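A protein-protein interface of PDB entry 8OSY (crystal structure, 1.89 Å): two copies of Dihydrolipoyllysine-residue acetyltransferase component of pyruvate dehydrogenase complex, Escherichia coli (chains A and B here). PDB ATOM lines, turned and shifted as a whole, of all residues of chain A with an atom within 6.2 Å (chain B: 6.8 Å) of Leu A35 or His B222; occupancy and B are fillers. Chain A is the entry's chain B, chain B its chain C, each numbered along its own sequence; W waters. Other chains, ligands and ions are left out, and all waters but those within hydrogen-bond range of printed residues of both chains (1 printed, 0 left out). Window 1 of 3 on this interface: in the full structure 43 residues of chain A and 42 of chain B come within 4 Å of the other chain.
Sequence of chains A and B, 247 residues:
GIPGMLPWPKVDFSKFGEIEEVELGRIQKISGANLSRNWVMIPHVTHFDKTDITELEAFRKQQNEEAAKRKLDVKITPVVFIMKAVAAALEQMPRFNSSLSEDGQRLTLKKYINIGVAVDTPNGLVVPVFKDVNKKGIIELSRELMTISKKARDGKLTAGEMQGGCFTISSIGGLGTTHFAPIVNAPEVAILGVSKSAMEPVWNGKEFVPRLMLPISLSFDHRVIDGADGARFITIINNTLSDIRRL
NE1 of Trp A39 lies within hydrogen-bond range of O of Ile B42 (3.1 Å).
The backbone carbonyl oxygen (O) of Gly A32 sits at hydrogen-bond distance from the side-chain hydroxyl (OG) of Ser A36, 3.2 Å away. N of Phe B220 is in hydrogen-bond range of O of Val B45, 2.9 Å away. O of Pro B43 sits at hydrogen-bond distance from N of His B222, at 2.9 Å. OD2 of Asp B221 is in salt-bridge range of NH2 of Arg B223, 2.8 Å away. The backbone carbonyl oxygen (O) of Ile B42 is in hydrogen-bond range of a ring nitrogen (ND1) of His B44 (2.8 Å). The backbone carbonyl oxygen (O) of Ile B225 lies within hydrogen-bond range of a ring nitrogen (ND1) of His B222, at 2.9 Å.
Gly A32 touches Arg B223 (O to CG, 3.9995 Å). Leu A35 touches Pro B43 (O to CG, 3.7 Å). CD1 of Leu A35 touches O of His B222, 3.4 Å away. Ser A36 touches Arg B223. Trp A39 touches Pro B43 (CG to CA, 3.6 Å). His B44 touches Trp A39 (O to CZ3, 3.6 Å). CD1 of Ile A183 touches CB of Pro B43 (3.7 Å). His B44 touches Ile A183. CG2 of Val B45 touches CD1 of Ile A183, 3.8 Å away. CD1 of Ile A183 touches CD2 of His B222, 3.8 Å away.
Leu A35 touches just these residues of chain B: Pro B43 (3.7 Å) and His B222 (3.4 Å). Of the printed residues of chain B, Ser A36 touches Arg B223. Arg A37 touches none of the printed residues of chain B. Printed residues of chain B within 4 Å of Ile A183: Pro B43 (3.7 Å), His B44 (3.4 Å), Val B45 (3.8 Å) and His B222 (3.8 Å). Printed residues of chain A within 4 Å of Pro B43: Leu A35, Trp A39 and Ile A183. Printed residues of chain A within 4 Å of His B44: Trp A39 (3.6 Å) and Ile A183 (3.4 Å). Of the printed residues of chain A, Val B45 touches Ile A183. Of chain A, only Leu A35 and Ile A183 come within 4 Å of His B222. The nearest printed residue of chain A that does not touch Arg B223 is Leu A35 (4.05 Å).
Printed residues of chain B that touch a printed residue of chain A: Ile B42, Pro B43, His B44, Val B45, His B222 and Arg B223. Hydrophobic or aromatic side chains of chain B within 4 Å of the printed part of chain A: Pro B43, His B44, Val B45 and His B222. Of the 13 printed residues of chain A, 5 touch a printed residue of chain B. Hydrophobic or aromatic side chains of chain A that line the printed part of chain B: Leu A35, Trp A39 and Ile A183. Among the printed residues, no Asp or Glu carboxylate lies within 4 Å of a Lys or Arg side-chain nitrogen of the other chain.
No position is printed for both chains.
Water W1 lies within hydrogen-bond range of N of Ile A183 (2.9 Å) and NE2 of His B222 (3.0 Å).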
ATOM      1  N   ILE A  30      21.508  34.640   7.664  1.00  0.00           N
ATOM      2  CA  ILE A  30      22.218  33.700   8.524  1.00  0.00           C
ATOM      3  C   ILE A  30      22.713  32.509   7.710  1.00  0.00           C
ATOM      4  O   ILE A  30      23.885  32.122   7.791  1.00  0.00           O
ATOM      5  CB  ILE A  30      21.313  33.264   9.692  1.00  0.00           C
ATOM      6  CG1 ILE A  30      21.146  34.417  10.678  1.00  0.00           C
ATOM      7  CG2 ILE A  30      21.879  32.041  10.391  1.00  0.00           C
ATOM      8  CD1 ILE A  30      19.877  34.328  11.515  1.00  0.00           C
ATOM      9  N   SER A  31      21.833  31.920   6.902  1.00  0.00           N
ATOM     10  CA  SER A  31      22.247  30.789   6.083  1.00  0.00           C
ATOM     11  C   SER A  31      23.326  31.196   5.084  1.00  0.00           C
ATOM     12  O   SER A  31      24.279  30.445   4.857  1.00  0.00           O
ATOM     13  CB  SER A  31      21.034  30.182   5.377  1.00  0.00           C
ATOM     14  OG  SER A  31      20.330  31.157   4.635  1.00  0.00           O
ATOM     15  N   GLY A  32      23.211  32.392   4.499  1.00  0.00           N
ATOM     16  CA  GLY A  32      24.245  32.864   3.594  1.00  0.00           C
ATOM     17  C   GLY A  32      25.595  33.046   4.265  1.00  0.00           C
ATOM     18  O   GLY A  32      26.638  32.800   3.650  1.00  0.00           O
ATOM     19  N   ALA A  33      25.601  33.485   5.528  1.00  0.00           N
ATOM     20  CA  ALA A  33      26.857  33.587   6.264  1.00  0.00           C
ATOM     21  C   ALA A  33      27.436  32.208   6.565  1.00  0.00           C
ATOM     22  O   ALA A  33      28.653  32.010   6.478  1.00  0.00           O
ATOM     23  CB  ALA A  33      26.655  34.377   7.555  1.00  0.00           C
ATOM     24  N   ASN A  34      26.584  31.245   6.927  1.00  0.00           N
ATOM     25  CA  ASN A  34      27.064  29.885   7.163  1.00  0.00           C
ATOM     26  C   ASN A  34      27.624  29.270   5.885  1.00  0.00           C
ATOM     27  O   ASN A  34      28.678  28.619   5.908  1.00  0.00           O
ATOM     28  CB  ASN A  34      25.936  29.016   7.724  1.00  0.00           C
ATOM     29  CG  ASN A  34      25.735  29.211   9.217  1.00  0.00           C
ATOM     30  OD1 ASN A  34      26.699  29.346   9.971  1.00  0.00           O
ATOM     31  ND2 ASN A  34      24.476  29.241   9.648  1.00  0.00           N
ATOM     32  N   LEU A  35      26.932  29.464   4.759  1.00  0.00           N
ATOM     33  CA  LEU A  35      27.413  28.923   3.489  1.00  0.00           C
ATOM     34  C   LEU A  35      28.766  29.506   3.106  1.00  0.00           C
ATOM     35  O   LEU A  35      29.627  28.795   2.580  1.00  0.00           O
ATOM     36  CB  LEU A  35      26.392  29.189   2.382  1.00  0.00           C
ATOM     37  CG  LEU A  35      25.180  28.266   2.392  1.00  0.00           C
ATOM     38  CD1 LEU A  35      24.146  28.734   1.389  1.00  0.00           C
ATOM     39  CD2 LEU A  35      25.636  26.833   2.094  1.00  0.00           C
ATOM     40  N   SER A  36      28.969  30.803   3.345  1.00  0.00           N
ATOM     41  CA  SER A  36      30.248  31.417   3.003  1.00  0.00           C
ATOM     42  C   SER A  36      31.382  30.803   3.816  1.00  0.00           C
ATOM     43  O   SER A  36      32.484  30.578   3.296  1.00  0.00           O
ATOM     44  CB  SER A  36      30.179  32.927   3.225  1.00  0.00           C
ATOM     45  OG  SER A  36      29.432  33.549   2.200  1.00  0.00           O
ATOM     46  N   ARG A  37      31.127  30.527   5.098  1.00  0.00           N
ATOM     47  CA  ARG A  37      32.116  29.867   5.944  1.00  0.00           C
ATOM     48  C   ARG A  37      32.327  28.418   5.524  1.00  0.00           C
ATOM     49  O   ARG A  37      33.466  27.977   5.329  1.00  0.00           O
ATOM     50  CB  ARG A  37      31.678  29.927   7.406  1.00  0.00           C
ATOM     51  CG  ARG A  37      32.602  29.162   8.336  1.00  0.00           C
ATOM     52  CD  ARG A  37      31.913  28.764   9.640  1.00  0.00           C
ATOM     53  NE  ARG A  37      30.809  27.838   9.417  1.00  0.00           N
ATOM     54  CZ  ARG A  37      29.643  27.895  10.044  1.00  0.00           C
ATOM     55  NH1 ARG A  37      29.398  28.814  10.967  1.00  0.00           N
ATOM     56  NH2 ARG A  37      28.697  27.009   9.737  1.00  0.00           N
ATOM     57  N   ASN A  38      31.237  27.656   5.413  1.00  0.00           N
ATOM     58  CA  ASN A  38      31.349  26.240   5.080  1.00  0.00           C
ATOM     59  C   ASN A  38      32.060  26.034   3.748  1.00  0.00           C
ATOM     60  O   ASN A  38      32.844  25.093   3.596  1.00  0.00           O
ATOM     61  CB  ASN A  38      29.961  25.604   5.045  1.00  0.00           C
ATOM     62  CG  ASN A  38      29.265  25.660   6.382  1.00  0.00           C
ATOM     63  OD1 ASN A  38      29.807  26.186   7.357  1.00  0.00           O
ATOM     64  ND2 ASN A  38      28.047  25.130   6.435  1.00  0.00           N
ATOM     65  N   TRP A  39      31.806  26.915   2.779  1.00  0.00           N
ATOM     66  CA  TRP A  39      32.331  26.723   1.435  1.00  0.00           C
ATOM     67  C   TRP A  39      33.851  26.817   1.406  1.00  0.00           C
ATOM     68  O   TRP A  39      34.516  26.004   0.746  1.00  0.00           O
ATOM     69  CB  TRP A  39      31.715  27.748   0.488  1.00  0.00           C
ATOM     70  CG  TRP A  39      32.221  27.647  -0.904  1.00  0.00           C
ATOM     71  CD1 TRP A  39      32.965  28.574  -1.566  1.00  0.00           C
ATOM     72  CD2 TRP A  39      32.020  26.559  -1.817  1.00  0.00           C
ATOM     73  NE1 TRP A  39      33.238  28.134  -2.837  1.00  0.00           N
ATOM     74  CE2 TRP A  39      32.678  26.897  -3.014  1.00  0.00           C
ATOM     75  CE3 TRP A  39      31.362  25.325  -1.732  1.00  0.00           C
ATOM     76  CZ2 TRP A  39      32.684  26.054  -4.127  1.00  0.00           C
ATOM     77  CZ3 TRP A  39      31.370  24.484  -2.848  1.00  0.00           C
ATOM     78  CH2 TRP A  39      32.029  24.854  -4.020  1.00  0.00           C
ATOM     79  N   VAL A  40      34.425  27.791   2.120  1.00  0.00           N
ATOM     80  CA  VAL A  40      35.871  27.973   2.043  1.00  0.00           C
ATOM     81  C   VAL A  40      36.616  27.027   2.983  1.00  0.00           C
ATOM     82  O   VAL A  40      37.776  26.702   2.731  1.00  0.00           O
ATOM     83  CB  VAL A  40      36.269  29.439   2.311  1.00  0.00           C
ATOM     84  CG1 VAL A  40      35.564  30.366   1.337  1.00  0.00           C
ATOM     85  CG2 VAL A  40      35.959  29.828   3.728  1.00  0.00           C
ATOM     86  N   ILE A 183      26.085  21.117  -1.075  1.00  0.00           N
ATOM     87  CA  ILE A 183      27.117  21.597  -0.161  1.00  0.00           C
ATOM     88  C   ILE A 183      26.920  20.955   1.207  1.00  0.00           C
ATOM     89  O   ILE A 183      25.789  20.813   1.684  1.00  0.00           O
ATOM     90  CB  ILE A 183      27.084  23.136  -0.080  1.00  0.00           C
ATOM     91  CG1 ILE A 183      27.711  23.718  -1.356  1.00  0.00           C
ATOM     92  CG2 ILE A 183      27.819  23.644   1.159  1.00  0.00           C
ATOM     93  CD1 ILE A 183      27.578  25.235  -1.506  1.00  0.00           C
ATOM     94  N   VAL A 184      28.032  20.599   1.855  1.00  0.00           N
ATOM     95  CA  VAL A 184      27.995  19.983   3.176  1.00  0.00           C
ATOM     96  C   VAL A 184      27.457  20.977   4.202  1.00  0.00           C
ATOM     97  O   VAL A 184      27.798  22.164   4.184  1.00  0.00           O
ATOM     98  CB  VAL A 184      29.401  19.492   3.563  1.00  0.00           C
ATOM     99  CG1 VAL A 184      29.402  18.903   4.967  1.00  0.00           C
ATOM    100  CG2 VAL A 184      29.911  18.467   2.551  1.00  0.00           C
ATOM    101  N   ILE B  42      31.756  32.683  -3.873  1.00  0.00           N
ATOM    102  CA  ILE B  42      30.467  32.127  -4.275  1.00  0.00           C
ATOM    103  C   ILE B  42      30.422  30.658  -3.858  1.00  0.00           C
ATOM    104  O   ILE B  42      31.151  29.837  -4.432  1.00  0.00           O
ATOM    105  CB  ILE B  42      30.222  32.267  -5.782  1.00  0.00           C
ATOM    106  CG1 ILE B  42      30.104  33.731  -6.179  1.00  0.00           C
ATOM    107  CG2 ILE B  42      28.961  31.525  -6.189  1.00  0.00           C
ATOM    108  CD1 ILE B  42      30.010  33.924  -7.671  1.00  0.00           C
ATOM    109  N   PRO B  43      29.573  30.276  -2.884  1.00  0.00           N
ATOM    110  CA  PRO B  43      29.338  28.849  -2.621  1.00  0.00           C
ATOM    111  C   PRO B  43      28.569  28.203  -3.761  1.00  0.00           C
ATOM    112  O   PRO B  43      27.388  28.499  -3.961  1.00  0.00           O
ATOM    113  CB  PRO B  43      28.521  28.855  -1.320  1.00  0.00           C
ATOM    114  CG  PRO B  43      28.785  30.237  -0.700  1.00  0.00           C
ATOM    115  CD  PRO B  43      28.927  31.143  -1.882  1.00  0.00           C
ATOM    116  N   HIS B  44      29.233  27.323  -4.511  1.00  0.00           N
ATOM    117  CA  HIS B  44      28.680  26.759  -5.734  1.00  0.00           C
ATOM    118  C   HIS B  44      27.876  25.503  -5.446  1.00  0.00           C
ATOM    119  O   HIS B  44      28.368  24.592  -4.777  1.00  0.00           O
ATOM    120  CB  HIS B  44      29.799  26.384  -6.710  1.00  0.00           C
ATOM    121  CG  HIS B  44      30.327  27.532  -7.497  1.00  0.00           C
ATOM    122  ND1 HIS B  44      30.960  28.606  -6.909  1.00  0.00           N
ATOM    123  CD2 HIS B  44      30.327  27.771  -8.829  1.00  0.00           C
ATOM    124  CE1 HIS B  44      31.329  29.456  -7.849  1.00  0.00           C
ATOM    125  NE2 HIS B  44      30.949  28.976  -9.020  1.00  0.00           N
ATOM    126  N   VAL B  45      26.677  25.424  -6.011  1.00  0.00           N
ATOM    127  CA  VAL B  45      25.988  24.146  -6.179  1.00  0.00           C
ATOM    128  C   VAL B  45      25.791  23.958  -7.675  1.00  0.00           C
ATOM    129  O   VAL B  45      25.549  24.927  -8.402  1.00  0.00           O
ATOM    130  CB  VAL B  45      24.624  24.097  -5.439  1.00  0.00           C
ATOM    131  CG1 VAL B  45      23.802  22.830  -5.829  1.00  0.00           C
ATOM    132  CG2 VAL B  45      24.805  24.201  -3.922  1.00  0.00           C
ATOM    133  N   VAL B 189      24.412  35.353 -10.735  1.00  0.00           N
ATOM    134  CA  VAL B 189      24.193  34.321  -9.728  1.00  0.00           C
ATOM    135  C   VAL B 189      24.123  32.910 -10.308  1.00  0.00           C
ATOM    136  O   VAL B 189      24.223  31.944  -9.533  1.00  0.00           O
ATOM    137  CB  VAL B 189      22.936  34.590  -8.874  1.00  0.00           C
ATOM    138  CG1 VAL B 189      23.078  35.892  -8.125  1.00  0.00           C
ATOM    139  CG2 VAL B 189      21.685  34.588  -9.728  1.00  0.00           C
ATOM    140  N   PHE B 220      25.136  27.624  -9.493  1.00  0.00           N
ATOM    141  CA  PHE B 220      24.505  28.824  -8.967  1.00  0.00           C
ATOM    142  C   PHE B 220      25.059  29.178  -7.594  1.00  0.00           C
ATOM    143  O   PHE B 220      25.600  28.335  -6.868  1.00  0.00           O
ATOM    144  CB  PHE B 220      22.974  28.674  -8.946  1.00  0.00           C
ATOM    145  CG  PHE B 220      22.460  27.458  -8.191  1.00  0.00           C
ATOM    146  CD1 PHE B 220      22.250  27.510  -6.818  1.00  0.00           C
ATOM    147  CD2 PHE B 220      22.134  26.293  -8.869  1.00  0.00           C
ATOM    148  CE1 PHE B 220      21.741  26.403  -6.124  1.00  0.00           C
ATOM    149  CE2 PHE B 220      21.631  25.176  -8.194  1.00  0.00           C
ATOM    150  CZ  PHE B 220      21.429  25.233  -6.817  1.00  0.00           C
ATOM    151  N   ASP B 221      24.946  30.465  -7.270  1.00  0.00           N
ATOM    152  CA  ASP B 221      25.330  31.003  -5.974  1.00  0.00           C
ATOM    153  C   ASP B 221      24.322  30.527  -4.932  1.00  0.00           C
ATOM    154  O   ASP B 221      23.162  30.957  -4.934  1.00  0.00           O
ATOM    155  CB  ASP B 221      25.374  32.532  -6.060  1.00  0.00           C
ATOM    156  CG  ASP B 221      26.032  33.183  -4.858  1.00  0.00           C
ATOM    157  OD1 ASP B 221      26.011  32.598  -3.757  1.00  0.00           O
ATOM    158  OD2 ASP B 221      26.583  34.301  -5.030  1.00  0.00           O
ATOM    159  N   HIS B 222      24.763  29.634  -4.045  1.00  0.00           N
ATOM    160  CA  HIS B 222      23.872  29.028  -3.059  1.00  0.00           C
ATOM    161  C   HIS B 222      23.421  30.022  -1.995  1.00  0.00           C
ATOM    162  O   HIS B 222      22.431  29.755  -1.304  1.00  0.00           O
ATOM    163  CB  HIS B 222      24.567  27.826  -2.401  1.00  0.00           C
ATOM    164  CG  HIS B 222      23.628  26.816  -1.810  1.00  0.00           C
ATOM    165  ND1 HIS B 222      22.301  26.721  -2.172  1.00  0.00           N
ATOM    166  CD2 HIS B 222      23.844  25.823  -0.911  1.00  0.00           C
ATOM    167  CE1 HIS B 222      21.734  25.729  -1.504  1.00  0.00           C
ATOM    168  NE2 HIS B 222      22.651  25.164  -0.738  1.00  0.00           N
ATOM    169  N   ARG B 223      24.117  31.162  -1.849  1.00  0.00           N
ATOM    170  CA  ARG B 223      23.627  32.211  -0.965  1.00  0.00           C
ATOM    171  C   ARG B 223      22.316  32.799  -1.469  1.00  0.00           C
ATOM    172  O   ARG B 223      21.563  33.369  -0.681  1.00  0.00           O
ATOM    173  CB  ARG B 223      24.663  33.335  -0.835  1.00  0.00           C
ATOM    174  CG  ARG B 223      26.033  32.909  -0.302  1.00  0.00           C
ATOM    175  CD  ARG B 223      27.035  34.073  -0.362  1.00  0.00           C
ATOM    176  NE  ARG B 223      27.301  34.493  -1.732  1.00  0.00           N
ATOM    177  CZ  ARG B 223      28.000  35.568  -2.072  1.00  0.00           C
ATOM    178  NH1 ARG B 223      28.522  36.375  -1.158  1.00  0.00           N
ATOM    179  NH2 ARG B 223      28.162  35.854  -3.360  1.00  0.00           N
ATOM    180  N   VAL B 224      22.042  32.684  -2.765  1.00  0.00           N
ATOM    181  CA  VAL B 224      20.872  33.298  -3.375  1.00  0.00           C
ATOM    182  C   VAL B 224      19.795  32.269  -3.695  1.00  0.00           C
ATOM    183  O   VAL B 224      18.607  32.515  -3.479  1.00  0.00           O
ATOM    184  CB  VAL B 224      21.296  34.071  -4.642  1.00  0.00           C
ATOM    185  CG1 VAL B 224      20.087  34.708  -5.321  1.00  0.00           C
ATOM    186  CG2 VAL B 224      22.342  35.123  -4.295  1.00  0.00           C
ATOM    187  N   ILE B 225      20.208  31.121  -4.213  1.00  0.00           N
ATOM    188  CA  ILE B 225      19.323  30.111  -4.775  1.00  0.00           C
ATOM    189  C   ILE B 225      19.461  28.843  -3.943  1.00  0.00           C
ATOM    190  O   ILE B 225      20.578  28.348  -3.766  1.00  0.00           O
ATOM    191  CB  ILE B 225      19.693  29.818  -6.244  1.00  0.00           C
ATOM    192  CG1 ILE B 225      19.652  31.095  -7.101  1.00  0.00           C
ATOM    193  CG2 ILE B 225      18.841  28.683  -6.803  1.00  0.00           C
ATOM    194  CD1 ILE B 225      18.270  31.777  -7.135  1.00  0.00           C
ATOM    195  N   ASP B 226      18.339  28.304  -3.453  1.00  0.00           N
ATOM    196  CA  ASP B 226      18.428  27.022  -2.759  1.00  0.00           C
ATOM    197  C   ASP B 226      18.232  25.861  -3.739  1.00  0.00           C
ATOM    198  O   ASP B 226      17.964  26.053  -4.927  1.00  0.00           O
ATOM    199  CB  ASP B 226      17.465  26.965  -1.555  1.00  0.00           C
ATOM    200  CG  ASP B 226      15.976  26.810  -1.923  1.00  0.00           C
ATOM    201  OD1 ASP B 226      15.596  26.464  -3.054  1.00  0.00           O
ATOM    202  OD2 ASP B 226      15.153  27.044  -1.012  1.00  0.00           O
ATOM    203  N   GLY B 227      18.428  24.640  -3.241  1.00  0.00           N
ATOM    204  CA  GLY B 227      18.444  23.494  -4.137  1.00  0.00           C
ATOM    205  C   GLY B 227      17.129  23.279  -4.860  1.00  0.00           C
ATOM    206  O   GLY B 227      17.111  22.831  -6.012  1.00  0.00           O
ATOM    207  N   ALA B 228      16.010  23.589  -4.196  1.00  0.00           N
ATOM    208  CA  ALA B 228      14.701  23.374  -4.800  1.00  0.00           C
ATOM    209  C   ALA B 228      14.434  24.375  -5.917  1.00  0.00           C
ATOM    210  O   ALA B 228      13.892  24.012  -6.963  1.00  0.00           O
ATOM    211  CB  ALA B 228      13.610  23.455  -3.725  1.00  0.00           C
HETATM  212  O   HOH W   1      23.442  22.259  -0.908  1.00  0.00           O
